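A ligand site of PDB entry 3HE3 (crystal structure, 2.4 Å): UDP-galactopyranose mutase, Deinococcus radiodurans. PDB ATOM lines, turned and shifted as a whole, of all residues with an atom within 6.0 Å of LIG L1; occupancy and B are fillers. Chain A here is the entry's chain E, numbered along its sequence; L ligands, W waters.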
ATOM      1  N   ALA A 113      29.102  25.706 -22.671  1.00  0.00           N
ATOM      2  CA  ALA A 113      28.503  26.991 -23.010  1.00  0.00           C
ATOM      3  C   ALA A 113      29.465  28.111 -22.660  1.00  0.00           C
ATOM      4  O   ALA A 113      29.981  28.178 -21.538  1.00  0.00           O
ATOM      5  CB  ALA A 113      27.196  27.178 -22.272  1.00  0.00           C
ATOM      6  N   ILE A 122      26.590  22.663 -19.782  1.00  0.00           N
ATOM      7  CA  ILE A 122      25.169  22.851 -20.027  1.00  0.00           C
ATOM      8  C   ILE A 122      24.678  21.478 -20.471  1.00  0.00           C
ATOM      9  O   ILE A 122      25.287  20.851 -21.328  1.00  0.00           O
ATOM     10  CB  ILE A 122      24.900  23.925 -21.113  1.00  0.00           C
ATOM     11  CG1 ILE A 122      23.403  24.221 -21.253  1.00  0.00           C
ATOM     12  CG2 ILE A 122      25.510  23.520 -22.457  1.00  0.00           C
ATOM     13  CD1 ILE A 122      22.933  25.392 -20.415  1.00  0.00           C
ATOM     14  N   PHE A 175      22.047  31.788 -19.550  1.00  0.00           N
ATOM     15  CA  PHE A 175      22.101  30.565 -20.342  1.00  0.00           C
ATOM     16  C   PHE A 175      20.960  30.407 -21.351  1.00  0.00           C
ATOM     17  O   PHE A 175      21.155  29.817 -22.414  1.00  0.00           O
ATOM     18  CB  PHE A 175      22.156  29.326 -19.429  1.00  0.00           C
ATOM     19  CG  PHE A 175      23.449  29.193 -18.669  1.00  0.00           C
ATOM     20  CD1 PHE A 175      23.644  29.871 -17.470  1.00  0.00           C
ATOM     21  CD2 PHE A 175      24.463  28.382 -19.141  1.00  0.00           C
ATOM     22  CE1 PHE A 175      24.831  29.757 -16.771  1.00  0.00           C
ATOM     23  CE2 PHE A 175      25.647  28.251 -18.439  1.00  0.00           C
ATOM     24  CZ  PHE A 175      25.833  28.937 -17.260  1.00  0.00           C
ATOM     25  N   PHE A 176      19.789  30.948 -21.033  1.00  0.00           N
ATOM     26  CA  PHE A 176      18.597  30.612 -21.814  1.00  0.00           C
ATOM     27  C   PHE A 176      18.002  31.761 -22.630  1.00  0.00           C
ATOM     28  O   PHE A 176      17.623  31.558 -23.786  1.00  0.00           O
ATOM     29  CB  PHE A 176      17.533  29.977 -20.927  1.00  0.00           C
ATOM     30  CG  PHE A 176      17.818  28.550 -20.570  1.00  0.00           C
ATOM     31  CD1 PHE A 176      17.477  27.529 -21.436  1.00  0.00           C
ATOM     32  CD2 PHE A 176      18.464  28.241 -19.384  1.00  0.00           C
ATOM     33  CE1 PHE A 176      17.754  26.214 -21.122  1.00  0.00           C
ATOM     34  CE2 PHE A 176      18.741  26.916 -19.060  1.00  0.00           C
ATOM     35  CZ  PHE A 176      18.387  25.907 -19.934  1.00  0.00           C
ATOM     36  N   ARG A 177      17.893  32.947 -22.036  1.00  0.00           N
ATOM     37  CA  ARG A 177      17.203  34.033 -22.720  1.00  0.00           C
ATOM     38  C   ARG A 177      17.843  34.451 -24.034  1.00  0.00           C
ATOM     39  O   ARG A 177      17.176  34.566 -25.061  1.00  0.00           O
ATOM     40  CB  ARG A 177      17.072  35.254 -21.809  1.00  0.00           C
ATOM     41  CG  ARG A 177      16.176  36.328 -22.395  1.00  0.00           C
ATOM     42  CD  ARG A 177      16.074  37.514 -21.485  1.00  0.00           C
ATOM     43  NE  ARG A 177      17.380  38.078 -21.173  1.00  0.00           N
ATOM     44  CZ  ARG A 177      17.596  39.358 -20.915  1.00  0.00           C
ATOM     45  NH1 ARG A 177      16.588  40.220 -20.942  1.00  0.00           N
ATOM     46  NH2 ARG A 177      18.823  39.794 -20.634  1.00  0.00           N
ATOM     47  N   TYR A 179      20.289  32.853 -25.907  1.00  0.00           N
ATOM     48  CA  TYR A 179      20.343  31.755 -26.851  1.00  0.00           C
ATOM     49  C   TYR A 179      19.000  31.603 -27.555  1.00  0.00           C
ATOM     50  O   TYR A 179      18.928  31.548 -28.780  1.00  0.00           O
ATOM     51  CB  TYR A 179      20.724  30.458 -26.136  1.00  0.00           C
ATOM     52  CG  TYR A 179      21.009  29.291 -27.053  1.00  0.00           C
ATOM     53  CD1 TYR A 179      22.308  28.880 -27.298  1.00  0.00           C
ATOM     54  CD2 TYR A 179      19.977  28.606 -27.688  1.00  0.00           C
ATOM     55  CE1 TYR A 179      22.570  27.814 -28.151  1.00  0.00           C
ATOM     56  CE2 TYR A 179      20.232  27.537 -28.535  1.00  0.00           C
ATOM     57  CZ  TYR A 179      21.531  27.153 -28.765  1.00  0.00           C
ATOM     58  OH  TYR A 179      21.790  26.098 -29.598  1.00  0.00           O
ATOM     59  N   THR A 180      17.940  31.546 -26.755  1.00  0.00           N
ATOM     60  CA  THR A 180      16.592  31.344 -27.266  1.00  0.00           C
ATOM     61  C   THR A 180      16.175  32.439 -28.250  1.00  0.00           C
ATOM     62  O   THR A 180      15.645  32.140 -29.326  1.00  0.00           O
ATOM     63  CB  THR A 180      15.566  31.284 -26.124  1.00  0.00           C
ATOM     64  OG1 THR A 180      15.969  30.296 -25.177  1.00  0.00           O
ATOM     65  CG2 THR A 180      14.190  30.921 -26.677  1.00  0.00           C
ATOM     66  N   GLN A 183      18.145  31.893 -31.358  1.00  0.00           N
ATOM     67  CA  GLN A 183      17.781  30.652 -32.051  1.00  0.00           C
ATOM     68  C   GLN A 183      16.397  30.711 -32.699  1.00  0.00           C
ATOM     69  O   GLN A 183      16.213  30.245 -33.831  1.00  0.00           O
ATOM     70  CB  GLN A 183      17.887  29.462 -31.103  1.00  0.00           C
ATOM     71  CG  GLN A 183      17.152  28.207 -31.579  1.00  0.00           C
ATOM     72  CD  GLN A 183      17.743  27.601 -32.848  1.00  0.00           C
ATOM     73  OE1 GLN A 183      18.595  28.207 -33.510  1.00  0.00           O
ATOM     74  NE2 GLN A 183      17.284  26.402 -33.190  1.00  0.00           N
ATOM     75  N   TRP A 184      15.432  31.285 -31.984  1.00  0.00           N
ATOM     76  CA  TRP A 184      14.038  31.260 -32.430  1.00  0.00           C
ATOM     77  C   TRP A 184      13.560  32.573 -33.038  1.00  0.00           C
ATOM     78  O   TRP A 184      12.686  32.582 -33.909  1.00  0.00           O
ATOM     79  CB  TRP A 184      13.124  30.851 -31.278  1.00  0.00           C
ATOM     80  CG  TRP A 184      13.359  29.454 -30.800  1.00  0.00           C
ATOM     81  CD1 TRP A 184      14.066  29.068 -29.702  1.00  0.00           C
ATOM     82  CD2 TRP A 184      12.877  28.257 -31.409  1.00  0.00           C
ATOM     83  NE1 TRP A 184      14.053  27.701 -29.584  1.00  0.00           N
ATOM     84  CE2 TRP A 184      13.335  27.180 -30.627  1.00  0.00           C
ATOM     85  CE3 TRP A 184      12.105  27.990 -32.546  1.00  0.00           C
ATOM     86  CZ2 TRP A 184      13.037  25.850 -30.941  1.00  0.00           C
ATOM     87  CZ3 TRP A 184      11.822  26.666 -32.855  1.00  0.00           C
ATOM     88  CH2 TRP A 184      12.281  25.617 -32.058  1.00  0.00           C
ATOM     89  N   LEU A 191       7.351  31.318 -26.359  1.00  0.00           N
ATOM     90  CA  LEU A 191       7.467  29.914 -26.731  1.00  0.00           C
ATOM     91  C   LEU A 191       6.868  28.965 -25.687  1.00  0.00           C
ATOM     92  O   LEU A 191       6.954  29.203 -24.486  1.00  0.00           O
ATOM     93  CB  LEU A 191       8.933  29.544 -26.972  1.00  0.00           C
ATOM     94  CG  LEU A 191       9.561  30.084 -28.262  1.00  0.00           C
ATOM     95  CD1 LEU A 191      11.062  29.954 -28.200  1.00  0.00           C
ATOM     96  CD2 LEU A 191       9.013  29.347 -29.476  1.00  0.00           C
ATOM     97  N   VAL A 195       9.773  23.824 -25.185  1.00  0.00           N
ATOM     98  CA  VAL A 195      11.023  24.124 -25.875  1.00  0.00           C
ATOM     99  C   VAL A 195      12.260  24.043 -24.955  1.00  0.00           C
ATOM    100  O   VAL A 195      13.129  23.198 -25.174  1.00  0.00           O
ATOM    101  CB  VAL A 195      10.955  25.479 -26.606  1.00  0.00           C
ATOM    102  CG1 VAL A 195      12.323  25.876 -27.138  1.00  0.00           C
ATOM    103  CG2 VAL A 195       9.941  25.403 -27.748  1.00  0.00           C
ATOM    104  N   THR A 196      12.345  24.907 -23.952  1.00  0.00           N
ATOM    105  CA  THR A 196      13.508  24.919 -23.064  1.00  0.00           C
ATOM    106  C   THR A 196      13.484  23.792 -22.034  1.00  0.00           C
ATOM    107  O   THR A 196      14.496  23.495 -21.410  1.00  0.00           O
ATOM    108  CB  THR A 196      13.649  26.257 -22.327  1.00  0.00           C
ATOM    109  OG1 THR A 196      12.557  26.421 -21.423  1.00  0.00           O
ATOM    110  CG2 THR A 196      13.670  27.413 -23.312  1.00  0.00           C
ATOM    111  N   ALA A 197      12.323  23.171 -21.860  1.00  0.00           N
ATOM    112  CA  ALA A 197      12.226  22.028 -20.970  1.00  0.00           C
ATOM    113  C   ALA A 197      13.062  20.867 -21.486  1.00  0.00           C
ATOM    114  O   ALA A 197      13.320  19.900 -20.771  1.00  0.00           O
ATOM    115  CB  ALA A 197      10.775  21.612 -20.801  1.00  0.00           C
ATOM    116  N   ARG A 198      13.492  20.969 -22.747  1.00  0.00           N
ATOM    117  CA  ARG A 198      14.376  19.965 -23.329  1.00  0.00           C
ATOM    118  C   ARG A 198      15.706  19.904 -22.599  1.00  0.00           C
ATOM    119  O   ARG A 198      16.282  18.831 -22.439  1.00  0.00           O
ATOM    120  CB  ARG A 198      14.619  20.246 -24.814  1.00  0.00           C
ATOM    121  CG  ARG A 198      13.469  19.830 -25.705  1.00  0.00           C
ATOM    122  CD  ARG A 198      13.595  20.488 -27.062  1.00  0.00           C
ATOM    123  NE  ARG A 198      14.788  20.054 -27.779  1.00  0.00           N
ATOM    124  CZ  ARG A 198      14.839  18.980 -28.568  1.00  0.00           C
ATOM    125  NH1 ARG A 198      13.755  18.231 -28.719  1.00  0.00           N
ATOM    126  NH2 ARG A 198      15.964  18.657 -29.186  1.00  0.00           N
ATOM    127  N   VAL A 199      16.200  21.050 -22.151  1.00  0.00           N
ATOM    128  CA  VAL A 199      17.473  21.124 -21.443  1.00  0.00           C
ATOM    129  C   VAL A 199      17.251  21.310 -19.944  1.00  0.00           C
ATOM    130  O   VAL A 199      17.358  22.423 -19.420  1.00  0.00           O
ATOM    131  CB  VAL A 199      18.343  22.278 -21.951  1.00  0.00           C
ATOM    132  CG1 VAL A 199      19.692  22.293 -21.237  1.00  0.00           C
ATOM    133  CG2 VAL A 199      18.526  22.172 -23.464  1.00  0.00           C
ATOM    134  N   TYR A 209      25.064  15.759 -22.260  1.00  0.00           N
ATOM    135  CA  TYR A 209      23.884  16.485 -22.719  1.00  0.00           C
ATOM    136  C   TYR A 209      22.660  15.579 -22.682  1.00  0.00           C
ATOM    137  O   TYR A 209      21.528  16.049 -22.618  1.00  0.00           O
ATOM    138  CB  TYR A 209      24.130  17.042 -24.127  1.00  0.00           C
ATOM    139  CG  TYR A 209      23.319  18.275 -24.461  1.00  0.00           C
ATOM    140  CD1 TYR A 209      23.521  19.471 -23.784  1.00  0.00           C
ATOM    141  CD2 TYR A 209      22.389  18.255 -25.494  1.00  0.00           C
ATOM    142  CE1 TYR A 209      22.783  20.613 -24.103  1.00  0.00           C
ATOM    143  CE2 TYR A 209      21.656  19.384 -25.815  1.00  0.00           C
ATOM    144  CZ  TYR A 209      21.854  20.553 -25.124  1.00  0.00           C
ATOM    145  OH  TYR A 209      21.119  21.676 -25.452  1.00  0.00           O
ATOM    146  N   ASN A 296      28.288  26.104 -27.109  1.00  0.00           N
ATOM    147  CA  ASN A 296      27.152  27.016 -27.284  1.00  0.00           C
ATOM    148  C   ASN A 296      27.529  28.466 -27.022  1.00  0.00           C
ATOM    149  O   ASN A 296      28.355  28.751 -26.152  1.00  0.00           O
ATOM    150  CB  ASN A 296      26.005  26.619 -26.355  1.00  0.00           C
ATOM    151  CG  ASN A 296      25.239  25.410 -26.857  1.00  0.00           C
ATOM    152  OD1 ASN A 296      25.537  24.862 -27.908  1.00  0.00           O
ATOM    153  ND2 ASN A 296      24.249  24.995 -26.083  1.00  0.00           N
ATOM    154  N   PRO A 298      25.470  31.533 -25.946  1.00  0.00           N
ATOM    155  CA  PRO A 298      24.225  32.151 -25.474  1.00  0.00           C
ATOM    156  C   PRO A 298      24.251  33.675 -25.601  1.00  0.00           C
ATOM    157  O   PRO A 298      23.216  34.270 -25.889  1.00  0.00           O
ATOM    158  CB  PRO A 298      24.189  31.767 -23.991  1.00  0.00           C
ATOM    159  CG  PRO A 298      25.145  30.637 -23.836  1.00  0.00           C
ATOM    160  CD  PRO A 298      26.207  30.877 -24.853  1.00  0.00           C
ATOM    161  N   ARG A 305      26.192  28.140 -32.042  1.00  0.00           N
ATOM    162  CA  ARG A 305      27.127  27.112 -31.595  1.00  0.00           C
ATOM    163  C   ARG A 305      28.081  26.654 -32.692  1.00  0.00           C
ATOM    164  O   ARG A 305      27.808  26.818 -33.876  1.00  0.00           O
ATOM    165  CB  ARG A 305      26.344  25.911 -31.079  1.00  0.00           C
ATOM    166  CG  ARG A 305      25.330  25.410 -32.091  1.00  0.00           C
ATOM    167  CD  ARG A 305      24.435  24.357 -31.472  1.00  0.00           C
ATOM    168  NE  ARG A 305      23.574  23.734 -32.477  1.00  0.00           N
ATOM    169  CZ  ARG A 305      22.640  22.848 -32.195  1.00  0.00           C
ATOM    170  NH1 ARG A 305      22.427  22.466 -30.944  1.00  0.00           N
ATOM    171  NH2 ARG A 305      21.889  22.334 -33.174  1.00  0.00           N
ATOM    172  N   GLU A 325      26.452  27.322 -36.771  1.00  0.00           N
ATOM    173  CA  GLU A 325      25.019  27.382 -37.038  1.00  0.00           C
ATOM    174  C   GLU A 325      24.430  28.782 -36.883  1.00  0.00           C
ATOM    175  O   GLU A 325      24.484  29.370 -35.796  1.00  0.00           O
ATOM    176  CB  GLU A 325      24.252  26.414 -36.130  1.00  0.00           C
ATOM    177  CG  GLU A 325      24.273  24.974 -36.613  1.00  0.00           C
ATOM    178  CD  GLU A 325      23.475  24.061 -35.693  1.00  0.00           C
ATOM    179  OE1 GLU A 325      24.043  23.060 -35.212  1.00  0.00           O
ATOM    180  OE2 GLU A 325      22.288  24.367 -35.445  1.00  0.00           O
ATOM    181  N   TYR A 335      12.894  23.428 -37.838  1.00  0.00           N
ATOM    182  CA  TYR A 335      12.211  23.393 -36.551  1.00  0.00           C
ATOM    183  C   TYR A 335      10.757  23.812 -36.656  1.00  0.00           C
ATOM    184  O   TYR A 335      10.445  24.875 -37.199  1.00  0.00           O
ATOM    185  CB  TYR A 335      12.896  24.328 -35.555  1.00  0.00           C
ATOM    186  CG  TYR A 335      14.309  23.955 -35.181  1.00  0.00           C
ATOM    187  CD1 TYR A 335      15.386  24.398 -35.937  1.00  0.00           C
ATOM    188  CD2 TYR A 335      14.577  23.171 -34.062  1.00  0.00           C
ATOM    189  CE1 TYR A 335      16.679  24.065 -35.597  1.00  0.00           C
ATOM    190  CE2 TYR A 335      15.863  22.835 -33.715  1.00  0.00           C
ATOM    191  CZ  TYR A 335      16.910  23.284 -34.485  1.00  0.00           C
ATOM    192  OH  TYR A 335      18.203  22.951 -34.145  1.00  0.00           O
ATOM    193  N   ARG A 364       8.888  14.714 -38.439  1.00  0.00           N
ATOM    194  CA  ARG A 364       9.035  15.962 -37.696  1.00  0.00           C
ATOM    195  C   ARG A 364       8.258  17.086 -38.377  1.00  0.00           C
ATOM    196  O   ARG A 364       7.526  17.826 -37.725  1.00  0.00           O
ATOM    197  CB  ARG A 364      10.507  16.353 -37.632  1.00  0.00           C
ATOM    198  CG  ARG A 364      10.807  17.432 -36.619  1.00  0.00           C
ATOM    199  CD  ARG A 364      12.209  17.985 -36.800  1.00  0.00           C
ATOM    200  NE  ARG A 364      12.919  18.010 -35.530  1.00  0.00           N
ATOM    201  CZ  ARG A 364      13.942  18.809 -35.259  1.00  0.00           C
ATOM    202  NH1 ARG A 364      14.380  19.650 -36.176  1.00  0.00           N
ATOM    203  NH2 ARG A 364      14.533  18.754 -34.074  1.00  0.00           N
ATOM    204  N   TYR A 370       8.458  18.573 -32.619  1.00  0.00           N
ATOM    205  CA  TYR A 370       9.868  18.814 -32.339  1.00  0.00           C
ATOM    206  C   TYR A 370      10.521  17.496 -31.875  1.00  0.00           C
ATOM    207  O   TYR A 370      10.861  17.349 -30.703  1.00  0.00           O
ATOM    208  CB  TYR A 370       9.974  19.910 -31.278  1.00  0.00           C
ATOM    209  CG  TYR A 370      11.344  20.524 -31.090  1.00  0.00           C
ATOM    210  CD1 TYR A 370      12.410  20.193 -31.907  1.00  0.00           C
ATOM    211  CD2 TYR A 370      11.561  21.480 -30.095  1.00  0.00           C
ATOM    212  CE1 TYR A 370      13.654  20.757 -31.729  1.00  0.00           C
ATOM    213  CE2 TYR A 370      12.793  22.054 -29.908  1.00  0.00           C
ATOM    214  CZ  TYR A 370      13.839  21.694 -30.733  1.00  0.00           C
ATOM    215  OH  TYR A 370      15.073  22.276 -30.539  1.00  0.00           O
HETATM  216  N1  LIG L   1      18.666  26.371 -24.934  1.00  0.00           N
HETATM  217  C1  LIG L   1      19.204  27.504 -24.364  1.00  0.00           C
HETATM  218  N2  LIG L   1      20.543  27.552 -24.031  1.00  0.00           N
HETATM  219  C2  LIG L   1      21.351  26.461 -24.264  1.00  0.00           C
HETATM  220  C3  LIG L   1      20.811  25.321 -24.841  1.00  0.00           C
HETATM  221  C4  LIG L   1      19.445  25.256 -25.085  1.00  0.00           C
HETATM  222  O1  LIG L   1      18.497  28.490 -24.156  1.00  0.00           O
HETATM  223  O2  LIG L   1      22.554  26.505 -23.957  1.00  0.00           O
HETATM  224  C5  LIG L   1      17.241  26.343 -25.290  1.00  0.00           C
HETATM  225  C6  LIG L   1      17.069  26.905 -26.684  1.00  0.00           C
HETATM  226  O3  LIG L   1      15.897  27.693 -26.743  1.00  0.00           O
HETATM  227  C7  LIG L   1      16.915  25.675 -27.552  1.00  0.00           C
HETATM  228  C8  LIG L   1      16.271  24.675 -26.604  1.00  0.00           C
HETATM  229  O4  LIG L   1      16.763  25.009 -25.326  1.00  0.00           O
HETATM  230  O5  LIG L   1      16.090  25.939 -28.659  1.00  0.00           O
HETATM  231  C9  LIG L   1      16.586  23.238 -26.961  1.00  0.00           C
HETATM  232  O6  LIG L   1      17.964  23.076 -27.218  1.00  0.00           O
HETATM  233  P1  LIG L   1      18.468  21.752 -27.975  1.00  0.00           P
HETATM  234  O7  LIG L   1      17.998  20.554 -27.249  1.00  0.00           O
HETATM  235  O8  LIG L   1      19.937  21.732 -28.129  1.00  0.00           O
HETATM  236  O9  LIG L   1      17.701  21.818 -29.402  1.00  0.00           O
HETATM  237  P2  LIG L   1      18.447  21.607 -30.806  1.00  0.00           P
HETATM  238  O10 LIG L   1      18.880  22.924 -31.330  1.00  0.00           O
HETATM  239  O11 LIG L   1      17.515  20.958 -31.759  1.00  0.00           O
HETATM  240  O12 LIG L   1      19.640  20.757 -30.611  1.00  0.00           O
HETATM  241  P1  LG2 L   2      13.571  14.940 -42.441  1.00  0.00           P
HETATM  242  O1  LG2 L   2      13.616  16.440 -42.609  1.00  0.00           O
HETATM  243  O2  LG2 L   2      14.907  14.408 -42.004  1.00  0.00           O
HETATM  244  O3  LG2 L   2      13.111  14.264 -43.827  1.00  0.00           O
HETATM  245  C1  LG2 L   2      12.239  14.935 -44.710  1.00  0.00           C
HETATM  246  C2  LG2 L   2      12.740  14.795 -46.141  1.00  0.00           C
HETATM  247  O4  LG2 L   2      11.661  14.945 -47.052  1.00  0.00           O
HETATM  248  C3  LG2 L   2      13.768  15.855 -46.492  1.00  0.00           C
HETATM  249  O5  LG2 L   2      14.971  15.241 -46.895  1.00  0.00           O
HETATM  250  C4  LG2 L   2      13.163  16.641 -47.636  1.00  0.00           C
HETATM  251  O6  LG2 L   2      14.110  16.913 -48.635  1.00  0.00           O
HETATM  252  C5  LG2 L   2      12.091  15.697 -48.173  1.00  0.00           C
HETATM  253  N1  LG2 L   2      10.990  16.435 -48.809  1.00  0.00           N
HETATM  254  C6  LG2 L   2      10.291  17.506 -48.287  1.00  0.00           C
HETATM  255  N2  LG2 L   2       9.365  17.897 -49.195  1.00  0.00           N
HETATM  256  C7  LG2 L   2       9.454  17.102 -50.285  1.00  0.00           C
HETATM  257  C8  LG2 L   2       8.765  17.065 -51.488  1.00  0.00           C
HETATM  258  N3  LG2 L   2       7.727  17.883 -51.670  1.00  0.00           N
HETATM  259  N4  LG2 L   2       9.087  16.129 -52.442  1.00  0.00           N
HETATM  260  C9  LG2 L   2      10.098  15.229 -52.192  1.00  0.00           C
HETATM  261  N5  LG2 L   2      10.792  15.262 -51.002  1.00  0.00           N
HETATM  262  C10 LG2 L   2      10.479  16.181 -50.063  1.00  0.00           C
HETATM  263  N6  LG2 L   2      18.076  14.494 -33.627  1.00  0.00           N
HETATM  264  C11 LG2 L   2      18.711  13.762 -32.643  1.00  0.00           C
HETATM  265  O7  LG2 L   2      18.214  12.711 -32.252  1.00  0.00           O
HETATM  266  N7  LG2 L   2      19.916  14.199 -32.113  1.00  0.00           N
HETATM  267  C12 LG2 L   2      20.486  15.367 -32.550  1.00  0.00           C
HETATM  268  O8  LG2 L   2      21.554  15.765 -32.069  1.00  0.00           O
HETATM  269  C13 LG2 L   2      19.846  16.112 -33.532  1.00  0.00           C
HETATM  270  N8  LG2 L   2      20.410  17.295 -33.984  1.00  0.00           N
HETATM  271  C14 LG2 L   2      19.776  18.025 -34.950  1.00  0.00           C
HETATM  272  C15 LG2 L   2      20.349  19.208 -35.391  1.00  0.00           C
HETATM  273  C16 LG2 L   2      19.732  19.962 -36.374  1.00  0.00           C
HETATM  274  C17 LG2 L   2      20.368  21.233 -36.840  1.00  0.00           C
HETATM  275  C18 LG2 L   2      18.526  19.527 -36.921  1.00  0.00           C
HETATM  276  C19 LG2 L   2      17.860  20.353 -37.983  1.00  0.00           C
HETATM  277  C20 LG2 L   2      17.939  18.346 -36.478  1.00  0.00           C
HETATM  278  C21 LG2 L   2      18.570  17.589 -35.497  1.00  0.00           C
HETATM  279  N9  LG2 L   2      18.006  16.407 -35.045  1.00  0.00           N
HETATM  280  C22 LG2 L   2      18.646  15.671 -34.074  1.00  0.00           C
HETATM  281  C23 LG2 L   2      16.568  16.087 -35.321  1.00  0.00           C
HETATM  282  C24 LG2 L   2      16.533  15.073 -36.450  1.00  0.00           C
HETATM  283  O9  LG2 L   2      17.124  15.658 -37.594  1.00  0.00           O
HETATM  284  C25 LG2 L   2      15.102  14.656 -36.757  1.00  0.00           C
HETATM  285  O10 LG2 L   2      14.625  13.853 -35.702  1.00  0.00           O
HETATM  286  C26 LG2 L   2      15.009  13.847 -38.045  1.00  0.00           C
HETATM  287  O11 LG2 L   2      15.570  14.567 -39.115  1.00  0.00           O
HETATM  288  C27 LG2 L   2      13.560  13.520 -38.386  1.00  0.00           C
HETATM  289  O12 LG2 L   2      13.534  13.028 -39.709  1.00  0.00           O
HETATM  290  P2  LG2 L   2      12.233  13.164 -40.637  1.00  0.00           P
HETATM  291  O13 LG2 L   2      12.229  12.025 -41.639  1.00  0.00           O
HETATM  292  O14 LG2 L   2      10.987  13.164 -39.791  1.00  0.00           O
HETATM  293  O15 LG2 L   2      12.400  14.588 -41.386  1.00  0.00           O
HETATM  294  O   HOH W   1      21.256  18.591 -29.375  1.00  0.00           O
HETATM  295  O   HOH W   2      16.629  24.517 -30.964  1.00  0.00           O
HETATM  296  O   HOH W   3      20.112  25.412 -31.643  1.00  0.00           O
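OG1 of Thr 180 is in hydrogen-bond range of O of Phe 176 (2.5 Å).
The guanidinium group (NE) of Arg 305 lies within salt-bridge range of the side-chain carboxylate (OE1) of Glu 325, at 2.9 Å.
O of Pro 298 lies within hydrogen-bond range of N of Tyr 179 (3.3 Å).
ND2 of Asn 296 sits at hydrogen-bond distance from O2 of LIG L1, at 3.1 Å.
O of Phe 175 lies within hydrogen-bond range of N2 of LIG L1 (2.8 Å).
The backbone NH (N) of Arg 364 sits at hydrogen-bond distance from an oxygen (O14) of LG2 L2, 2.9 Å away.
An oxygen (O8) of LIG L1 is in hydrogen-bond range of the side-chain hydroxyl (OH) of Tyr 209.
The side-chain hydroxyl (OH) of Tyr 335 sits at hydrogen-bond distance from an oxygen (O10) of LIG L1 (2.9 Å).
The indole nitrogen (NE1) of Trp 184 sits at hydrogen-bond distance from an oxygen (O5) of LIG L1 (2.8 Å).
An oxygen (O7) of LIG L1 lies within salt-bridge range of the guanidinium group of Arg 198.
OG1 of Thr 180 lies within hydrogen-bond range of O3 of LIG L1, 3.0 Å away.
NH1 of Arg 305 is in salt-bridge range of O12 of LIG L1, at 3.3 Å.
An oxygen (O9) of LIG L1 sits at hydrogen-bond distance from the side-chain hydroxyl of Tyr 370, 2.9 Å away.
The backbone carbonyl oxygen (O) of Phe 176 sits close to an oxygen (O1) of LIG L1, at 3.2 Å.
Residues that only touch LIG L1: Tyr 179, Val 199, Ile 122, Val 195, Gln 183 and Thr 196.
Water W2 lies within hydrogen-bond range of the side-chain hydroxyl (OH) of Tyr 370 (2.8 Å), an oxygen (O5) of LIG L1 (2.8 Å) and the side-chain amide nitrogen (NE2) of Gln 183 (3.0 Å).
Water W3 lies within hydrogen-bond range of OH of Tyr 179 (2.7 Å), O10 of LIG L1 (2.8 Å) and NE2 of Gln 183 (3.4 Å).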
